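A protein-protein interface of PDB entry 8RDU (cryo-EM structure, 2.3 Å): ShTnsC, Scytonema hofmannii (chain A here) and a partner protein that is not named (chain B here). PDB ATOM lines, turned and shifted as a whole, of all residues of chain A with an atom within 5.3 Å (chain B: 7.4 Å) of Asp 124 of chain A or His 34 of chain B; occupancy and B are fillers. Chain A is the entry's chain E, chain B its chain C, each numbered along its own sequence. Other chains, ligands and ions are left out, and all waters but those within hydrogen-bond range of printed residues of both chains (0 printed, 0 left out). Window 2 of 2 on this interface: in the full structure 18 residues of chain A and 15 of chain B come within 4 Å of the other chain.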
ATOM      1  N   GLY A 120      -1.842  -0.622  35.412  1.00  0.00           N
ATOM      2  CA  GLY A 120      -3.198  -0.175  35.672  1.00  0.00           C
ATOM      3  C   GLY A 120      -4.003  -1.270  36.334  1.00  0.00           C
ATOM      4  O   GLY A 120      -3.553  -2.401  36.497  1.00  0.00           O
ATOM      5  N   THR A 121      -5.212  -0.903  36.748  1.00  0.00           N
ATOM      6  CA  THR A 121      -6.141  -1.867  37.317  1.00  0.00           C
ATOM      7  C   THR A 121      -6.637  -2.843  36.250  1.00  0.00           C
ATOM      8  O   THR A 121      -6.483  -2.630  35.045  1.00  0.00           O
ATOM      9  CB  THR A 121      -7.319  -1.154  37.978  1.00  0.00           C
ATOM     10  OG1 THR A 121      -8.111  -0.501  36.979  1.00  0.00           O
ATOM     11  CG2 THR A 121      -6.820  -0.126  38.972  1.00  0.00           C
ATOM     12  N   VAL A 122      -7.237  -3.939  36.720  1.00  0.00           N
ATOM     13  CA  VAL A 122      -7.924  -4.879  35.836  1.00  0.00           C
ATOM     14  C   VAL A 122      -9.015  -4.186  35.028  1.00  0.00           C
ATOM     15  O   VAL A 122      -9.256  -4.529  33.865  1.00  0.00           O
ATOM     16  CB  VAL A 122      -8.490  -6.054  36.650  1.00  0.00           C
ATOM     17  CG1 VAL A 122      -9.106  -7.090  35.731  1.00  0.00           C
ATOM     18  CG2 VAL A 122      -7.395  -6.679  37.484  1.00  0.00           C
ATOM     19  N   SER A 123      -9.696  -3.208  35.627  1.00  0.00           N
ATOM     20  CA  SER A 123     -10.706  -2.452  34.893  1.00  0.00           C
ATOM     21  C   SER A 123     -10.093  -1.626  33.770  1.00  0.00           C
ATOM     22  O   SER A 123     -10.632  -1.584  32.659  1.00  0.00           O
ATOM     23  CB  SER A 123     -11.479  -1.552  35.853  1.00  0.00           C
ATOM     24  OG  SER A 123     -11.915  -2.284  36.982  1.00  0.00           O
ATOM     25  N   ASP A 124      -8.976  -0.952  34.040  1.00  0.00           N
ATOM     26  CA  ASP A 124      -8.271  -0.240  32.981  1.00  0.00           C
ATOM     27  C   ASP A 124      -7.734  -1.194  31.925  1.00  0.00           C
ATOM     28  O   ASP A 124      -7.866  -0.935  30.724  1.00  0.00           O
ATOM     29  CB  ASP A 124      -7.145   0.608  33.569  1.00  0.00           C
ATOM     30  CG  ASP A 124      -7.614   1.476  34.716  1.00  0.00           C
ATOM     31  OD1 ASP A 124      -8.705   2.071  34.594  1.00  0.00           O
ATOM     32  OD2 ASP A 124      -6.892   1.572  35.732  1.00  0.00           O
ATOM     33  N   PHE A 125      -7.133  -2.306  32.350  1.00  0.00           N
ATOM     34  CA  PHE A 125      -6.630  -3.289  31.395  1.00  0.00           C
ATOM     35  C   PHE A 125      -7.739  -3.873  30.531  1.00  0.00           C
ATOM     36  O   PHE A 125      -7.534  -4.115  29.340  1.00  0.00           O
ATOM     37  CB  PHE A 125      -5.880  -4.399  32.122  1.00  0.00           C
ATOM     38  CG  PHE A 125      -4.397  -4.208  32.146  1.00  0.00           C
ATOM     39  CD1 PHE A 125      -3.646  -4.419  31.004  1.00  0.00           C
ATOM     40  CD2 PHE A 125      -3.750  -3.820  33.306  1.00  0.00           C
ATOM     41  CE1 PHE A 125      -2.279  -4.249  31.016  1.00  0.00           C
ATOM     42  CE2 PHE A 125      -2.383  -3.649  33.327  1.00  0.00           C
ATOM     43  CZ  PHE A 125      -1.645  -3.864  32.180  1.00  0.00           C
ATOM     44  N   ARG A 126      -8.917  -4.117  31.107  1.00  0.00           N
ATOM     45  CA  ARG A 126     -10.046  -4.547  30.287  1.00  0.00           C
ATOM     46  C   ARG A 126     -10.406  -3.494  29.247  1.00  0.00           C
ATOM     47  O   ARG A 126     -10.476  -3.784  28.049  1.00  0.00           O
ATOM     48  CB  ARG A 126     -11.256  -4.868  31.169  1.00  0.00           C
ATOM     49  CG  ARG A 126     -12.425  -5.440  30.389  1.00  0.00           C
ATOM     50  CD  ARG A 126     -13.613  -5.818  31.259  1.00  0.00           C
ATOM     51  NE  ARG A 126     -13.356  -6.966  32.119  1.00  0.00           N
ATOM     52  CZ  ARG A 126     -13.008  -6.892  33.395  1.00  0.00           C
ATOM     53  NH1 ARG A 126     -12.995  -5.740  34.044  1.00  0.00           N
ATOM     54  NH2 ARG A 126     -12.709  -8.008  34.051  1.00  0.00           N
ATOM     55  N   ASP A 127     -10.649  -2.263  29.695  1.00  0.00           N
ATOM     56  CA  ASP A 127     -11.111  -1.200  28.807  1.00  0.00           C
ATOM     57  C   ASP A 127     -10.081  -0.852  27.737  1.00  0.00           C
ATOM     58  O   ASP A 127     -10.434  -0.624  26.574  1.00  0.00           O
ATOM     59  CB  ASP A 127     -11.465   0.033  29.633  1.00  0.00           C
ATOM     60  CG  ASP A 127     -12.639  -0.209  30.559  1.00  0.00           C
ATOM     61  OD1 ASP A 127     -13.336  -1.231  30.380  1.00  0.00           O
ATOM     62  OD2 ASP A 127     -12.859   0.615  31.470  1.00  0.00           O
ATOM     63  N   ARG A 128      -8.805  -0.796  28.114  1.00  0.00           N
ATOM     64  CA  ARG A 128      -7.737  -0.608  27.137  1.00  0.00           C
ATOM     65  C   ARG A 128      -7.624  -1.773  26.161  1.00  0.00           C
ATOM     66  O   ARG A 128      -7.362  -1.564  24.973  1.00  0.00           O
ATOM     67  CB  ARG A 128      -6.413  -0.373  27.863  1.00  0.00           C
ATOM     68  CG  ARG A 128      -6.425   0.911  28.660  1.00  0.00           C
ATOM     69  CD  ARG A 128      -5.123   1.196  29.373  1.00  0.00           C
ATOM     70  NE  ARG A 128      -4.564   0.060  30.086  1.00  0.00           N
ATOM     71  CZ  ARG A 128      -3.893   0.164  31.222  1.00  0.00           C
ATOM     72  NH1 ARG A 128      -3.860   1.297  31.902  1.00  0.00           N
ATOM     73  NH2 ARG A 128      -3.279  -0.909  31.714  1.00  0.00           N
ATOM     74  N   THR A 129      -7.812  -3.002  26.634  1.00  0.00           N
ATOM     75  CA  THR A 129      -7.726  -4.155  25.743  1.00  0.00           C
ATOM     76  C   THR A 129      -8.838  -4.153  24.700  1.00  0.00           C
ATOM     77  O   THR A 129      -8.587  -4.379  23.512  1.00  0.00           O
ATOM     78  CB  THR A 129      -7.769  -5.445  26.557  1.00  0.00           C
ATOM     79  OG1 THR A 129      -6.663  -5.464  27.464  1.00  0.00           O
ATOM     80  CG2 THR A 129      -7.695  -6.652  25.652  1.00  0.00           C
ATOM     81  N   GLU A 131     -10.499  -1.582  23.636  1.00  0.00           N
ATOM     82  CA  GLU A 131     -10.196  -0.480  22.728  1.00  0.00           C
ATOM     83  C   GLU A 131      -9.055  -0.809  21.770  1.00  0.00           C
ATOM     84  O   GLU A 131      -9.118  -0.471  20.584  1.00  0.00           O
ATOM     85  CB  GLU A 131      -9.862   0.772  23.538  1.00  0.00           C
ATOM     86  CG  GLU A 131      -9.926   2.064  22.752  1.00  0.00           C
ATOM     87  CD  GLU A 131     -11.321   2.369  22.247  1.00  0.00           C
ATOM     88  OE1 GLU A 131     -12.297   1.870  22.847  1.00  0.00           O
ATOM     89  OE2 GLU A 131     -11.445   3.107  21.246  1.00  0.00           O
ATOM     90  N   PHE B  12      -2.200   5.330  21.912  1.00  0.00           N
ATOM     91  CA  PHE B  12      -3.228   6.153  21.288  1.00  0.00           C
ATOM     92  C   PHE B  12      -2.873   7.627  21.431  1.00  0.00           C
ATOM     93  O   PHE B  12      -2.594   8.107  22.533  1.00  0.00           O
ATOM     94  CB  PHE B  12      -4.605   5.877  21.886  1.00  0.00           C
ATOM     95  CG  PHE B  12      -5.131   4.503  21.597  1.00  0.00           C
ATOM     96  CD1 PHE B  12      -5.550   4.167  20.320  1.00  0.00           C
ATOM     97  CD2 PHE B  12      -5.249   3.561  22.600  1.00  0.00           C
ATOM     98  CE1 PHE B  12      -6.046   2.912  20.045  1.00  0.00           C
ATOM     99  CE2 PHE B  12      -5.747   2.304  22.330  1.00  0.00           C
ATOM    100  CZ  PHE B  12      -6.148   1.980  21.050  1.00  0.00           C
ATOM    101  N   ARG B  28      -7.913  14.474  27.807  1.00  0.00           N
ATOM    102  CA  ARG B  28      -8.244  13.698  26.616  1.00  0.00           C
ATOM    103  C   ARG B  28      -7.259  12.557  26.391  1.00  0.00           C
ATOM    104  O   ARG B  28      -7.661  11.426  26.102  1.00  0.00           O
ATOM    105  CB  ARG B  28      -8.290  14.608  25.391  1.00  0.00           C
ATOM    106  CG  ARG B  28      -9.457  15.555  25.361  1.00  0.00           C
ATOM    107  CD  ARG B  28      -9.754  16.013  23.950  1.00  0.00           C
ATOM    108  NE  ARG B  28      -8.621  16.701  23.342  1.00  0.00           N
ATOM    109  CZ  ARG B  28      -8.228  16.524  22.091  1.00  0.00           C
ATOM    110  NH1 ARG B  28      -8.805  15.632  21.305  1.00  0.00           N
ATOM    111  NH2 ARG B  28      -7.215  17.245  21.621  1.00  0.00           N
ATOM    112  N   PHE B  29      -5.961  12.839  26.510  1.00  0.00           N
ATOM    113  CA  PHE B  29      -4.957  11.793  26.340  1.00  0.00           C
ATOM    114  C   PHE B  29      -5.123  10.678  27.363  1.00  0.00           C
ATOM    115  O   PHE B  29      -4.953   9.497  27.044  1.00  0.00           O
ATOM    116  CB  PHE B  29      -3.553  12.385  26.436  1.00  0.00           C
ATOM    117  CG  PHE B  29      -2.465  11.401  26.119  1.00  0.00           C
ATOM    118  CD1 PHE B  29      -2.040  11.216  24.817  1.00  0.00           C
ATOM    119  CD2 PHE B  29      -1.873  10.653  27.121  1.00  0.00           C
ATOM    120  CE1 PHE B  29      -1.050  10.309  24.520  1.00  0.00           C
ATOM    121  CE2 PHE B  29      -0.881   9.745  26.828  1.00  0.00           C
ATOM    122  CZ  PHE B  29      -0.471   9.576  25.526  1.00  0.00           C
ATOM    123  N   ARG B  30      -5.440  11.037  28.603  1.00  0.00           N
ATOM    124  CA  ARG B  30      -5.709  10.039  29.629  1.00  0.00           C
ATOM    125  C   ARG B  30      -6.949   9.210  29.316  1.00  0.00           C
ATOM    126  O   ARG B  30      -6.940   7.987  29.485  1.00  0.00           O
ATOM    127  CB  ARG B  30      -5.848  10.732  30.977  1.00  0.00           C
ATOM    128  CG  ARG B  30      -4.520  11.147  31.562  1.00  0.00           C
ATOM    129  CD  ARG B  30      -4.580  11.303  33.062  1.00  0.00           C
ATOM    130  NE  ARG B  30      -5.582  12.273  33.483  1.00  0.00           N
ATOM    131  CZ  ARG B  30      -6.779  11.958  33.955  1.00  0.00           C
ATOM    132  NH1 ARG B  30      -7.221  10.714  33.939  1.00  0.00           N
ATOM    133  NH2 ARG B  30      -7.568  12.923  34.416  1.00  0.00           N
ATOM    134  N   ARG B  31      -8.032   9.853  28.880  1.00  0.00           N
ATOM    135  CA  ARG B  31      -9.227   9.105  28.500  1.00  0.00           C
ATOM    136  C   ARG B  31      -8.994   8.223  27.279  1.00  0.00           C
ATOM    137  O   ARG B  31      -9.483   7.090  27.228  1.00  0.00           O
ATOM    138  CB  ARG B  31     -10.381  10.068  28.239  1.00  0.00           C
ATOM    139  CG  ARG B  31     -11.027  10.610  29.494  1.00  0.00           C
ATOM    140  CD  ARG B  31     -12.348  11.269  29.179  1.00  0.00           C
ATOM    141  NE  ARG B  31     -12.203  12.441  28.328  1.00  0.00           N
ATOM    142  CZ  ARG B  31     -11.762  13.622  28.738  1.00  0.00           C
ATOM    143  NH1 ARG B  31     -11.455  13.844  30.004  1.00  0.00           N
ATOM    144  NH2 ARG B  31     -11.636  14.607  27.856  1.00  0.00           N
ATOM    145  N   ALA B  32      -8.255   8.722  26.285  1.00  0.00           N
ATOM    146  CA  ALA B  32      -7.912   7.910  25.120  1.00  0.00           C
ATOM    147  C   ALA B  32      -7.128   6.657  25.480  1.00  0.00           C
ATOM    148  O   ALA B  32      -7.164   5.680  24.727  1.00  0.00           O
ATOM    149  CB  ALA B  32      -7.114   8.742  24.117  1.00  0.00           C
ATOM    150  N   ASN B  33      -6.430   6.659  26.611  1.00  0.00           N
ATOM    151  CA  ASN B  33      -5.645   5.515  27.048  1.00  0.00           C
ATOM    152  C   ASN B  33      -6.126   4.934  28.370  1.00  0.00           C
ATOM    153  O   ASN B  33      -5.408   4.132  28.969  1.00  0.00           O
ATOM    154  CB  ASN B  33      -4.167   5.897  27.149  1.00  0.00           C
ATOM    155  CG  ASN B  33      -3.567   6.246  25.804  1.00  0.00           C
ATOM    156  OD1 ASN B  33      -3.303   5.371  24.986  1.00  0.00           O
ATOM    157  ND2 ASN B  33      -3.348   7.531  25.569  1.00  0.00           N
ATOM    158  N   HIS B  34      -7.309   5.325  28.840  1.00  0.00           N
ATOM    159  CA  HIS B  34      -7.819   4.973  30.168  1.00  0.00           C
ATOM    160  C   HIS B  34      -6.736   5.030  31.243  1.00  0.00           C
ATOM    161  O   HIS B  34      -6.544   4.096  32.021  1.00  0.00           O
ATOM    162  CB  HIS B  34      -8.487   3.599  30.149  1.00  0.00           C
ATOM    163  CG  HIS B  34      -9.499   3.432  29.061  1.00  0.00           C
ATOM    164  ND1 HIS B  34      -9.154   3.159  27.756  1.00  0.00           N
ATOM    165  CD2 HIS B  34     -10.851   3.500  29.085  1.00  0.00           C
ATOM    166  CE1 HIS B  34     -10.248   3.070  27.022  1.00  0.00           C
ATOM    167  NE2 HIS B  34     -11.292   3.271  27.806  1.00  0.00           N
ATOM    168  N   LEU B  35      -6.001   6.139  31.262  1.00  0.00           N
ATOM    169  CA  LEU B  35      -4.970   6.384  32.261  1.00  0.00           C
ATOM    170  C   LEU B  35      -5.548   7.214  33.400  1.00  0.00           C
ATOM    171  O   LEU B  35      -6.271   8.185  33.165  1.00  0.00           O
ATOM    172  CB  LEU B  35      -3.773   7.109  31.651  1.00  0.00           C
ATOM    173  CG  LEU B  35      -2.970   6.352  30.599  1.00  0.00           C
ATOM    174  CD1 LEU B  35      -1.963   7.271  29.945  1.00  0.00           C
ATOM    175  CD2 LEU B  35      -2.277   5.179  31.242  1.00  0.00           C
ATOM    176  N   SER B  36      -5.237   6.829  34.634  1.00  0.00           N
ATOM    177  CA  SER B  36      -5.408   7.751  35.744  1.00  0.00           C
ATOM    178  C   SER B  36      -4.336   8.836  35.719  1.00  0.00           C
ATOM    179  O   SER B  36      -3.283   8.698  35.093  1.00  0.00           O
ATOM    180  CB  SER B  36      -5.355   7.009  37.079  1.00  0.00           C
ATOM    181  OG  SER B  36      -6.410   6.074  37.187  1.00  0.00           O
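His 34 of chain B touches Asp 124 of chain A (O to CB, 3.9 Å).
Asp 127 of chain A touches His 34 of chain B.
Asn 33 of chain B touches Arg 128 of chain A (O to CD, 3.0 Å).
CG of Arg 128 of chain A touches ND1 of His 34 of chain B, at 3.6 Å.
Phe 12 of chain B touches Glu 131 of chain A.
Asp 124 of chain A touches one residue of chain B.
Printed residues of chain B within 4 Å of Asp 127 of chain A: His 34 (3.6 Å).
Of the printed residues of chain B, Glu 131 of chain A touches Phe 12 (3.9 Å).
Of the printed residues of chain A, Phe 12 of chain B touches Glu 131.
Of the printed residues of chain A, Asn 33 of chain B touches Arg 128 (3.0 Å).
Printed residues of chain A within 4 Å of His 34 of chain B: Asp 124, Asp 127 and Arg 128.
Leu 35 of chain B touches none of the printed residues of chain A.
The nearest residue of chain A that does not touch His 34 of chain B is Glu 131 of chain A (4.2 Å).
The nearest printed residue of chain A that does not touch Phe 12 of chain B is Arg 128 of chain A (5.0 Å).
The backbone carbonyl oxygen (O) of Phe 12 of chain B lies within hydrogen-bond range of the side-chain amide nitrogen (ND2) of Asn 33 of chain B (3.2 Å).
OG1 of Thr 121 of chain A is in hydrogen-bond range of OD2 of Asp 124 of chain A (2.7 Å).
The side-chain amide nitrogen (ND2) of Asn 33 of chain B lies within hydrogen-bond range of the backbone carbonyl oxygen (O) of Phe 29 of chain B, 2.9 Å away.
Of the 10 printed residues of chain B, 3 touch a printed residue of chain A.
Hydrophobic or aromatic side chains of chain B within 4 Å of the printed part of chain A: Phe 12 and His 34.
Along chain B the printed residues that touch a printed residue of chain A span positions 12 to 34.
Among the printed residues, no Asp or Glu carboxylate lies within 4 Å of a Lys or Arg side-chain nitrogen of the other chain.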
